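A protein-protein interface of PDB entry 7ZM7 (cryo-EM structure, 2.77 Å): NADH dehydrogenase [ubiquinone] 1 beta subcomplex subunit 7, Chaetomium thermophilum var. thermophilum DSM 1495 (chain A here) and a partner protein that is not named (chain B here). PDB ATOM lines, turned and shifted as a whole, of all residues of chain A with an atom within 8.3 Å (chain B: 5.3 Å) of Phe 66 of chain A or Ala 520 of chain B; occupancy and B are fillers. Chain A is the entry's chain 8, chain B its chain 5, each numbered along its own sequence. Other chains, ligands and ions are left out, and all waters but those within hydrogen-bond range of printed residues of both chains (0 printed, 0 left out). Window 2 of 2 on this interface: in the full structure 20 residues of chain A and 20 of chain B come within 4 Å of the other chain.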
ATOM      1  N   SER A  29       1.265  22.019 -27.107  1.00  0.00           N
ATOM      2  CA  SER A  29       1.558  23.431 -26.907  1.00  0.00           C
ATOM      3  C   SER A  29       1.538  23.824 -25.438  1.00  0.00           C
ATOM      4  O   SER A  29       2.221  24.775 -25.045  1.00  0.00           O
ATOM      5  CB  SER A  29       0.549  24.270 -27.683  1.00  0.00           C
ATOM      6  OG  SER A  29      -0.762  24.031 -27.199  1.00  0.00           O
ATOM      7  N   CYS A  30       0.755  23.125 -24.619  1.00  0.00           N
ATOM      8  CA  CYS A  30       0.583  23.469 -23.215  1.00  0.00           C
ATOM      9  C   CYS A  30       1.185  22.431 -22.277  1.00  0.00           C
ATOM     10  O   CYS A  30       0.574  22.090 -21.262  1.00  0.00           O
ATOM     11  CB  CYS A  30      -0.898  23.674 -22.906  1.00  0.00           C
ATOM     12  SG  CYS A  30      -1.940  22.253 -23.278  1.00  0.00           S
ATOM     13  N   GLU A  59      -4.317  20.962 -15.554  1.00  0.00           N
ATOM     14  CA  GLU A  59      -5.638  20.676 -16.100  1.00  0.00           C
ATOM     15  C   GLU A  59      -6.297  21.931 -16.653  1.00  0.00           C
ATOM     16  O   GLU A  59      -6.898  21.898 -17.733  1.00  0.00           O
ATOM     17  CB  GLU A  59      -6.531  20.025 -15.046  1.00  0.00           C
ATOM     18  CG  GLU A  59      -6.108  18.625 -14.628  1.00  0.00           C
ATOM     19  CD  GLU A  59      -7.022  18.029 -13.572  1.00  0.00           C
ATOM     20  OE1 GLU A  59      -7.910  18.750 -13.074  1.00  0.00           O
ATOM     21  OE2 GLU A  59      -6.861  16.834 -13.246  1.00  0.00           O
ATOM     22  N   LYS A  60      -6.201  23.046 -15.926  1.00  0.00           N
ATOM     23  CA  LYS A  60      -6.843  24.279 -16.372  1.00  0.00           C
ATOM     24  C   LYS A  60      -6.280  24.746 -17.705  1.00  0.00           C
ATOM     25  O   LYS A  60      -7.033  25.166 -18.590  1.00  0.00           O
ATOM     26  CB  LYS A  60      -6.678  25.371 -15.318  1.00  0.00           C
ATOM     27  CG  LYS A  60      -7.395  26.668 -15.642  1.00  0.00           C
ATOM     28  CD  LYS A  60      -7.476  27.569 -14.423  1.00  0.00           C
ATOM     29  CE  LYS A  60      -7.869  28.985 -14.805  1.00  0.00           C
ATOM     30  NZ  LYS A  60      -6.791  29.665 -15.568  1.00  0.00           N
ATOM     31  N   CYS A  61      -4.958  24.689 -17.866  1.00  0.00           N
ATOM     32  CA  CYS A  61      -4.362  25.121 -19.123  1.00  0.00           C
ATOM     33  C   CYS A  61      -4.801  24.220 -20.268  1.00  0.00           C
ATOM     34  O   CYS A  61      -5.234  24.706 -21.318  1.00  0.00           O
ATOM     35  CB  CYS A  61      -2.841  25.142 -19.000  1.00  0.00           C
ATOM     36  SG  CYS A  61      -1.993  25.852 -20.420  1.00  0.00           S
ATOM     37  N   GLN A  62      -4.729  22.902 -20.069  1.00  0.00           N
ATOM     38  CA  GLN A  62      -5.185  21.964 -21.086  1.00  0.00           C
ATOM     39  C   GLN A  62      -6.670  22.116 -21.354  1.00  0.00           C
ATOM     40  O   GLN A  62      -7.153  21.751 -22.431  1.00  0.00           O
ATOM     41  CB  GLN A  62      -4.877  20.530 -20.658  1.00  0.00           C
ATOM     42  CG  GLN A  62      -3.531  20.025 -21.099  1.00  0.00           C
ATOM     43  CD  GLN A  62      -3.585  19.441 -22.487  1.00  0.00           C
ATOM     44  OE1 GLN A  62      -4.641  19.408 -23.114  1.00  0.00           O
ATOM     45  NE2 GLN A  62      -2.443  18.986 -22.986  1.00  0.00           N
ATOM     46  N   TYR A  63      -7.420  22.625 -20.381  1.00  0.00           N
ATOM     47  CA  TYR A  63      -8.839  22.858 -20.610  1.00  0.00           C
ATOM     48  C   TYR A  63      -9.049  23.906 -21.688  1.00  0.00           C
ATOM     49  O   TYR A  63      -9.904  23.740 -22.564  1.00  0.00           O
ATOM     50  CB  TYR A  63      -9.521  23.283 -19.310  1.00  0.00           C
ATOM     51  CG  TYR A  63     -11.025  23.379 -19.407  1.00  0.00           C
ATOM     52  CD1 TYR A  63     -11.806  22.240 -19.519  1.00  0.00           C
ATOM     53  CD2 TYR A  63     -11.662  24.607 -19.392  1.00  0.00           C
ATOM     54  CE1 TYR A  63     -13.179  22.326 -19.609  1.00  0.00           C
ATOM     55  CE2 TYR A  63     -13.034  24.703 -19.482  1.00  0.00           C
ATOM     56  CZ  TYR A  63     -13.788  23.559 -19.589  1.00  0.00           C
ATOM     57  OH  TYR A  63     -15.154  23.649 -19.680  1.00  0.00           O
ATOM     58  N   LEU A  64      -8.260  24.982 -21.656  1.00  0.00           N
ATOM     59  CA  LEU A  64      -8.488  26.098 -22.567  1.00  0.00           C
ATOM     60  C   LEU A  64      -8.274  25.693 -24.018  1.00  0.00           C
ATOM     61  O   LEU A  64      -9.099  26.006 -24.883  1.00  0.00           O
ATOM     62  CB  LEU A  64      -7.578  27.268 -22.198  1.00  0.00           C
ATOM     63  CG  LEU A  64      -7.872  27.957 -20.864  1.00  0.00           C
ATOM     64  CD1 LEU A  64      -7.224  29.331 -20.816  1.00  0.00           C
ATOM     65  CD2 LEU A  64      -9.368  28.063 -20.635  1.00  0.00           C
ATOM     66  N   GLU A  65      -7.181  24.986 -24.309  1.00  0.00           N
ATOM     67  CA  GLU A  65      -6.928  24.603 -25.692  1.00  0.00           C
ATOM     68  C   GLU A  65      -7.889  23.540 -26.194  1.00  0.00           C
ATOM     69  O   GLU A  65      -7.892  23.255 -27.396  1.00  0.00           O
ATOM     70  CB  GLU A  65      -5.488  24.125 -25.874  1.00  0.00           C
ATOM     71  CG  GLU A  65      -4.479  25.256 -25.963  1.00  0.00           C
ATOM     72  CD  GLU A  65      -3.816  25.550 -24.640  1.00  0.00           C
ATOM     73  OE1 GLU A  65      -4.004  24.756 -23.699  1.00  0.00           O
ATOM     74  OE2 GLU A  65      -3.111  26.576 -24.539  1.00  0.00           O
ATOM     75  N   PHE A  66      -8.692  22.945 -25.318  1.00  0.00           N
ATOM     76  CA  PHE A  66      -9.729  22.031 -25.766  1.00  0.00           C
ATOM     77  C   PHE A  66     -10.984  22.782 -26.187  1.00  0.00           C
ATOM     78  O   PHE A  66     -11.528  22.527 -27.266  1.00  0.00           O
ATOM     79  CB  PHE A  66     -10.050  21.023 -24.663  1.00  0.00           C
ATOM     80  CG  PHE A  66     -11.346  20.306 -24.857  1.00  0.00           C
ATOM     81  CD1 PHE A  66     -11.447  19.268 -25.757  1.00  0.00           C
ATOM     82  CD2 PHE A  66     -12.460  20.667 -24.138  1.00  0.00           C
ATOM     83  CE1 PHE A  66     -12.637  18.606 -25.934  1.00  0.00           C
ATOM     84  CE2 PHE A  66     -13.654  20.010 -24.315  1.00  0.00           C
ATOM     85  CZ  PHE A  66     -13.742  18.977 -25.210  1.00  0.00           C
ATOM     86  N   LYS A  67     -11.458  23.709 -25.353  1.00  0.00           N
ATOM     87  CA  LYS A  67     -12.639  24.477 -25.728  1.00  0.00           C
ATOM     88  C   LYS A  67     -12.362  25.353 -26.938  1.00  0.00           C
ATOM     89  O   LYS A  67     -13.285  25.670 -27.696  1.00  0.00           O
ATOM     90  CB  LYS A  67     -13.128  25.318 -24.549  1.00  0.00           C
ATOM     91  CG  LYS A  67     -12.355  26.599 -24.326  1.00  0.00           C
ATOM     92  CD  LYS A  67     -12.959  27.410 -23.194  1.00  0.00           C
ATOM     93  CE  LYS A  67     -14.300  28.002 -23.592  1.00  0.00           C
ATOM     94  NZ  LYS A  67     -14.853  28.871 -22.519  1.00  0.00           N
ATOM     95  N   LYS A  68     -11.105  25.748 -27.142  1.00  0.00           N
ATOM     96  CA  LYS A  68     -10.748  26.438 -28.372  1.00  0.00           C
ATOM     97  C   LYS A  68     -10.922  25.523 -29.574  1.00  0.00           C
ATOM     98  O   LYS A  68     -11.391  25.958 -30.632  1.00  0.00           O
ATOM     99  CB  LYS A  68      -9.313  26.950 -28.285  1.00  0.00           C
ATOM    100  CG  LYS A  68      -8.892  27.805 -29.459  1.00  0.00           C
ATOM    101  CD  LYS A  68      -7.465  28.281 -29.294  1.00  0.00           C
ATOM    102  CE  LYS A  68      -7.371  29.318 -28.192  1.00  0.00           C
ATOM    103  NZ  LYS A  68      -8.076  30.577 -28.552  1.00  0.00           N
ATOM    104  N   ARG A  69     -10.550  24.252 -29.431  1.00  0.00           N
ATOM    105  CA  ARG A  69     -10.775  23.298 -30.505  1.00  0.00           C
ATOM    106  C   ARG A  69     -12.260  23.043 -30.702  1.00  0.00           C
ATOM    107  O   ARG A  69     -12.722  22.872 -31.836  1.00  0.00           O
ATOM    108  CB  ARG A  69     -10.039  21.992 -30.215  1.00  0.00           C
ATOM    109  CG  ARG A  69      -8.526  22.094 -30.315  1.00  0.00           C
ATOM    110  CD  ARG A  69      -7.892  20.736 -30.521  1.00  0.00           C
ATOM    111  NE  ARG A  69      -8.220  19.808 -29.442  1.00  0.00           N
ATOM    112  CZ  ARG A  69      -7.590  19.766 -28.274  1.00  0.00           C
ATOM    113  NH1 ARG A  69      -7.957  18.892 -27.353  1.00  0.00           N
ATOM    114  NH2 ARG A  69      -6.595  20.603 -28.025  1.00  0.00           N
ATOM    115  N   VAL A  70     -13.026  23.017 -29.610  1.00  0.00           N
ATOM    116  CA  VAL A  70     -14.466  22.805 -29.717  1.00  0.00           C
ATOM    117  C   VAL A  70     -15.113  23.943 -30.489  1.00  0.00           C
ATOM    118  O   VAL A  70     -16.022  23.726 -31.301  1.00  0.00           O
ATOM    119  CB  VAL A  70     -15.090  22.648 -28.319  1.00  0.00           C
ATOM    120  CG1 VAL A  70     -16.604  22.609 -28.415  1.00  0.00           C
ATOM    121  CG2 VAL A  70     -14.573  21.393 -27.656  1.00  0.00           C
ATOM    122  N   GLN A  71     -14.660  25.174 -30.249  1.00  0.00           N
ATOM    123  CA  GLN A  71     -15.282  26.326 -30.892  1.00  0.00           C
ATOM    124  C   GLN A  71     -15.131  26.265 -32.405  1.00  0.00           C
ATOM    125  O   GLN A  71     -16.117  26.359 -33.143  1.00  0.00           O
ATOM    126  CB  GLN A  71     -14.680  27.620 -30.350  1.00  0.00           C
ATOM    127  CG  GLN A  71     -15.333  28.873 -30.904  1.00  0.00           C
ATOM    128  CD  GLN A  71     -14.758  30.142 -30.312  1.00  0.00           C
ATOM    129  OE1 GLN A  71     -13.834  30.100 -29.501  1.00  0.00           O
ATOM    130  NE2 GLN A  71     -15.306  31.282 -30.712  1.00  0.00           N
ATOM    131  N   LYS A  72     -13.901  26.101 -32.891  1.00  0.00           N
ATOM    132  CA  LYS A  72     -13.677  26.255 -34.323  1.00  0.00           C
ATOM    133  C   LYS A  72     -14.014  24.966 -35.065  1.00  0.00           C
ATOM    134  O   LYS A  72     -14.135  24.953 -36.294  1.00  0.00           O
ATOM    135  CB  LYS A  72     -12.241  26.718 -34.586  1.00  0.00           C
ATOM    136  N   MET A  73     -14.161  23.865 -34.328  1.00  0.00           N
ATOM    137  CA  MET A  73     -14.780  22.678 -34.905  1.00  0.00           C
ATOM    138  C   MET A  73     -16.234  22.940 -35.270  1.00  0.00           C
ATOM    139  O   MET A  73     -16.707  22.492 -36.321  1.00  0.00           O
ATOM    140  CB  MET A  73     -14.681  21.504 -33.937  1.00  0.00           C
ATOM    141  CG  MET A  73     -15.166  20.189 -34.517  1.00  0.00           C
ATOM    142  SD  MET A  73     -14.142  19.593 -35.871  1.00  0.00           S
ATOM    143  CE  MET A  73     -15.311  18.544 -36.730  1.00  0.00           C
ATOM    144  N   PHE B 403     -14.363   9.361 -30.206  1.00  0.00           N
ATOM    145  CA  PHE B 403     -15.602   9.645 -30.928  1.00  0.00           C
ATOM    146  C   PHE B 403     -15.556   8.980 -32.297  1.00  0.00           C
ATOM    147  O   PHE B 403     -15.288   9.601 -33.328  1.00  0.00           O
ATOM    148  CB  PHE B 403     -15.821  11.144 -31.037  1.00  0.00           C
ATOM    149  CG  PHE B 403     -16.418  11.744 -29.814  1.00  0.00           C
ATOM    150  CD1 PHE B 403     -17.783  11.834 -29.666  1.00  0.00           C
ATOM    151  CD2 PHE B 403     -15.609  12.188 -28.789  1.00  0.00           C
ATOM    152  CE1 PHE B 403     -18.333  12.376 -28.535  1.00  0.00           C
ATOM    153  CE2 PHE B 403     -16.154  12.730 -27.652  1.00  0.00           C
ATOM    154  CZ  PHE B 403     -17.519  12.824 -27.525  1.00  0.00           C
ATOM    155  N   ILE B 515      -7.451  13.432 -23.142  1.00  0.00           N
ATOM    156  CA  ILE B 515      -7.966  14.795 -23.076  1.00  0.00           C
ATOM    157  C   ILE B 515      -9.448  14.824 -23.411  1.00  0.00           C
ATOM    158  O   ILE B 515     -10.233  15.502 -22.741  1.00  0.00           O
ATOM    159  CB  ILE B 515      -7.165  15.720 -24.001  1.00  0.00           C
ATOM    160  CG1 ILE B 515      -5.688  15.692 -23.623  1.00  0.00           C
ATOM    161  CG2 ILE B 515      -7.695  17.129 -23.905  1.00  0.00           C
ATOM    162  CD1 ILE B 515      -5.424  16.165 -22.220  1.00  0.00           C
ATOM    163  N   ASP B 516      -9.857  14.103 -24.451  1.00  0.00           N
ATOM    164  CA  ASP B 516     -11.272  14.074 -24.797  1.00  0.00           C
ATOM    165  C   ASP B 516     -12.089  13.403 -23.703  1.00  0.00           C
ATOM    166  O   ASP B 516     -13.138  13.914 -23.298  1.00  0.00           O
ATOM    167  CB  ASP B 516     -11.468  13.361 -26.135  1.00  0.00           C
ATOM    168  CG  ASP B 516     -11.096  14.236 -27.311  1.00  0.00           C
ATOM    169  OD1 ASP B 516     -10.891  15.446 -27.097  1.00  0.00           O
ATOM    170  OD2 ASP B 516     -11.014  13.720 -28.445  1.00  0.00           O
ATOM    171  N   THR B 517     -11.616  12.264 -23.203  1.00  0.00           N
ATOM    172  CA  THR B 517     -12.327  11.577 -22.135  1.00  0.00           C
ATOM    173  C   THR B 517     -12.391  12.427 -20.875  1.00  0.00           C
ATOM    174  O   THR B 517     -13.324  12.288 -20.078  1.00  0.00           O
ATOM    175  CB  THR B 517     -11.659  10.232 -21.852  1.00  0.00           C
ATOM    176  OG1 THR B 517     -11.614   9.470 -23.058  1.00  0.00           O
ATOM    177  CG2 THR B 517     -12.426   9.454 -20.806  1.00  0.00           C
ATOM    178  N   GLU B 518     -11.425  13.322 -20.686  1.00  0.00           N
ATOM    179  CA  GLU B 518     -11.468  14.216 -19.538  1.00  0.00           C
ATOM    180  C   GLU B 518     -12.476  15.342 -19.721  1.00  0.00           C
ATOM    181  O   GLU B 518     -13.056  15.812 -18.736  1.00  0.00           O
ATOM    182  CB  GLU B 518     -10.079  14.796 -19.279  1.00  0.00           C
ATOM    183  CG  GLU B 518      -9.952  15.557 -17.971  1.00  0.00           C
ATOM    184  CD  GLU B 518     -10.084  14.659 -16.759  1.00  0.00           C
ATOM    185  OE1 GLU B 518      -9.765  13.456 -16.872  1.00  0.00           O
ATOM    186  OE2 GLU B 518     -10.501  15.154 -15.691  1.00  0.00           O
ATOM    187  N   PHE B 519     -12.707  15.785 -20.955  1.00  0.00           N
ATOM    188  CA  PHE B 519     -13.476  16.999 -21.188  1.00  0.00           C
ATOM    189  C   PHE B 519     -14.635  16.827 -22.151  1.00  0.00           C
ATOM    190  O   PHE B 519     -15.667  17.474 -21.977  1.00  0.00           O
ATOM    191  CB  PHE B 519     -12.565  18.108 -21.716  1.00  0.00           C
ATOM    192  CG  PHE B 519     -11.519  18.552 -20.741  1.00  0.00           C
ATOM    193  CD1 PHE B 519     -11.801  18.624 -19.392  1.00  0.00           C
ATOM    194  CD2 PHE B 519     -10.261  18.915 -21.178  1.00  0.00           C
ATOM    195  CE1 PHE B 519     -10.840  19.035 -18.498  1.00  0.00           C
ATOM    196  CE2 PHE B 519      -9.297  19.325 -20.288  1.00  0.00           C
ATOM    197  CZ  PHE B 519      -9.587  19.388 -18.947  1.00  0.00           C
ATOM    198  N   ALA B 520     -14.494  15.985 -23.173  1.00  0.00           N
ATOM    199  CA  ALA B 520     -15.490  15.965 -24.240  1.00  0.00           C
ATOM    200  C   ALA B 520     -16.781  15.291 -23.800  1.00  0.00           C
ATOM    201  O   ALA B 520     -17.873  15.729 -24.181  1.00  0.00           O
ATOM    202  CB  ALA B 520     -14.922  15.269 -25.474  1.00  0.00           C
ATOM    203  N   VAL B 521     -16.684  14.234 -23.006  1.00  0.00           N
ATOM    204  CA  VAL B 521     -17.864  13.416 -22.700  1.00  0.00           C
ATOM    205  C   VAL B 521     -18.863  14.242 -21.900  1.00  0.00           C
ATOM    206  O   VAL B 521     -18.458  14.997 -20.999  1.00  0.00           O
ATOM    207  CB  VAL B 521     -17.455  12.155 -21.938  1.00  0.00           C
ATOM    208  CG1 VAL B 521     -16.766  11.173 -22.870  1.00  0.00           C
ATOM    209  CG2 VAL B 521     -16.545  12.510 -20.778  1.00  0.00           C
ATOM    210  N   PRO B 522     -20.155  14.153 -22.196  1.00  0.00           N
ATOM    211  CA  PRO B 522     -21.149  14.849 -21.380  1.00  0.00           C
ATOM    212  C   PRO B 522     -21.349  14.151 -20.045  1.00  0.00           C
ATOM    213  O   PRO B 522     -20.995  12.986 -19.859  1.00  0.00           O
ATOM    214  CB  PRO B 522     -22.416  14.788 -22.236  1.00  0.00           C
ATOM    215  CG  PRO B 522     -22.239  13.561 -23.058  1.00  0.00           C
ATOM    216  CD  PRO B 522     -20.766  13.424 -23.319  1.00  0.00           C
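Among the printed residues, pairs that only touch across the chains: Glu 59 of chain A with Phe 519 of chain B (3.9 Å), Gln 62 of chain A with Ile 515 of chain B (3.5 Å), Gln 62 of chain A with Phe 519 of chain B (3.9 Å), Tyr 63 of chain A with Phe 519 of chain B (3.5 Å), Phe 66 of chain A with Asp 516 of chain B (3.8 Å), Phe 66 of chain A with Phe 519 of chain B (3.4 Å), Phe 66 of chain A with Ala 520 of chain B (3.6 Å) and Arg 69 of chain A with Ile 515 of chain B (3.9 Å).
Of the printed residues of chain B, Glu 59 of chain A touches Phe 519.
Printed residues of chain B within 4 Å of Tyr 63 of chain A: Phe 519.
Glu 65 of chain A touches none of the printed residues of chain B.
Phe 66 of chain A touches just these residues of chain B: Asp 516 (3.8 Å), Phe 519 (3.4 Å) and Ala 520 (3.6 Å).
Of the printed residues of chain B, Arg 69 of chain A touches Ile 515.
Printed residues of chain A within 4 Å of Ile 515 of chain B: Gln 62 and Arg 69.
Of the printed residues of chain A, Asp 516 of chain B touches Phe 66.
Ala 520 of chain B touches just one residue of chain A: Phe 66 (3.6 Å).
No residue of chain A comes within 4 Å of Val 521 of chain B.
The nearest printed residue of chain A that does not touch Asp 516 of chain B is Arg 69 of chain A (4.5 Å).
The side-chain sulfur (SG) of Cys 30 of chain A lies within hydrogen-bond range of the side-chain amide nitrogen (NE2) of Gln 62 of chain A (3.3 Å).
O of Glu 65 of chain A lies within hydrogen-bond range of NH2 of Arg 69 of chain A, at 3.0 Å.
Hydrophobic or aromatic side chains of chain B within 4 Å of the printed part of chain A: Ile 515, Phe 519 and Ala 520.
Among the printed residues, 8 pairs touch across the chains.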
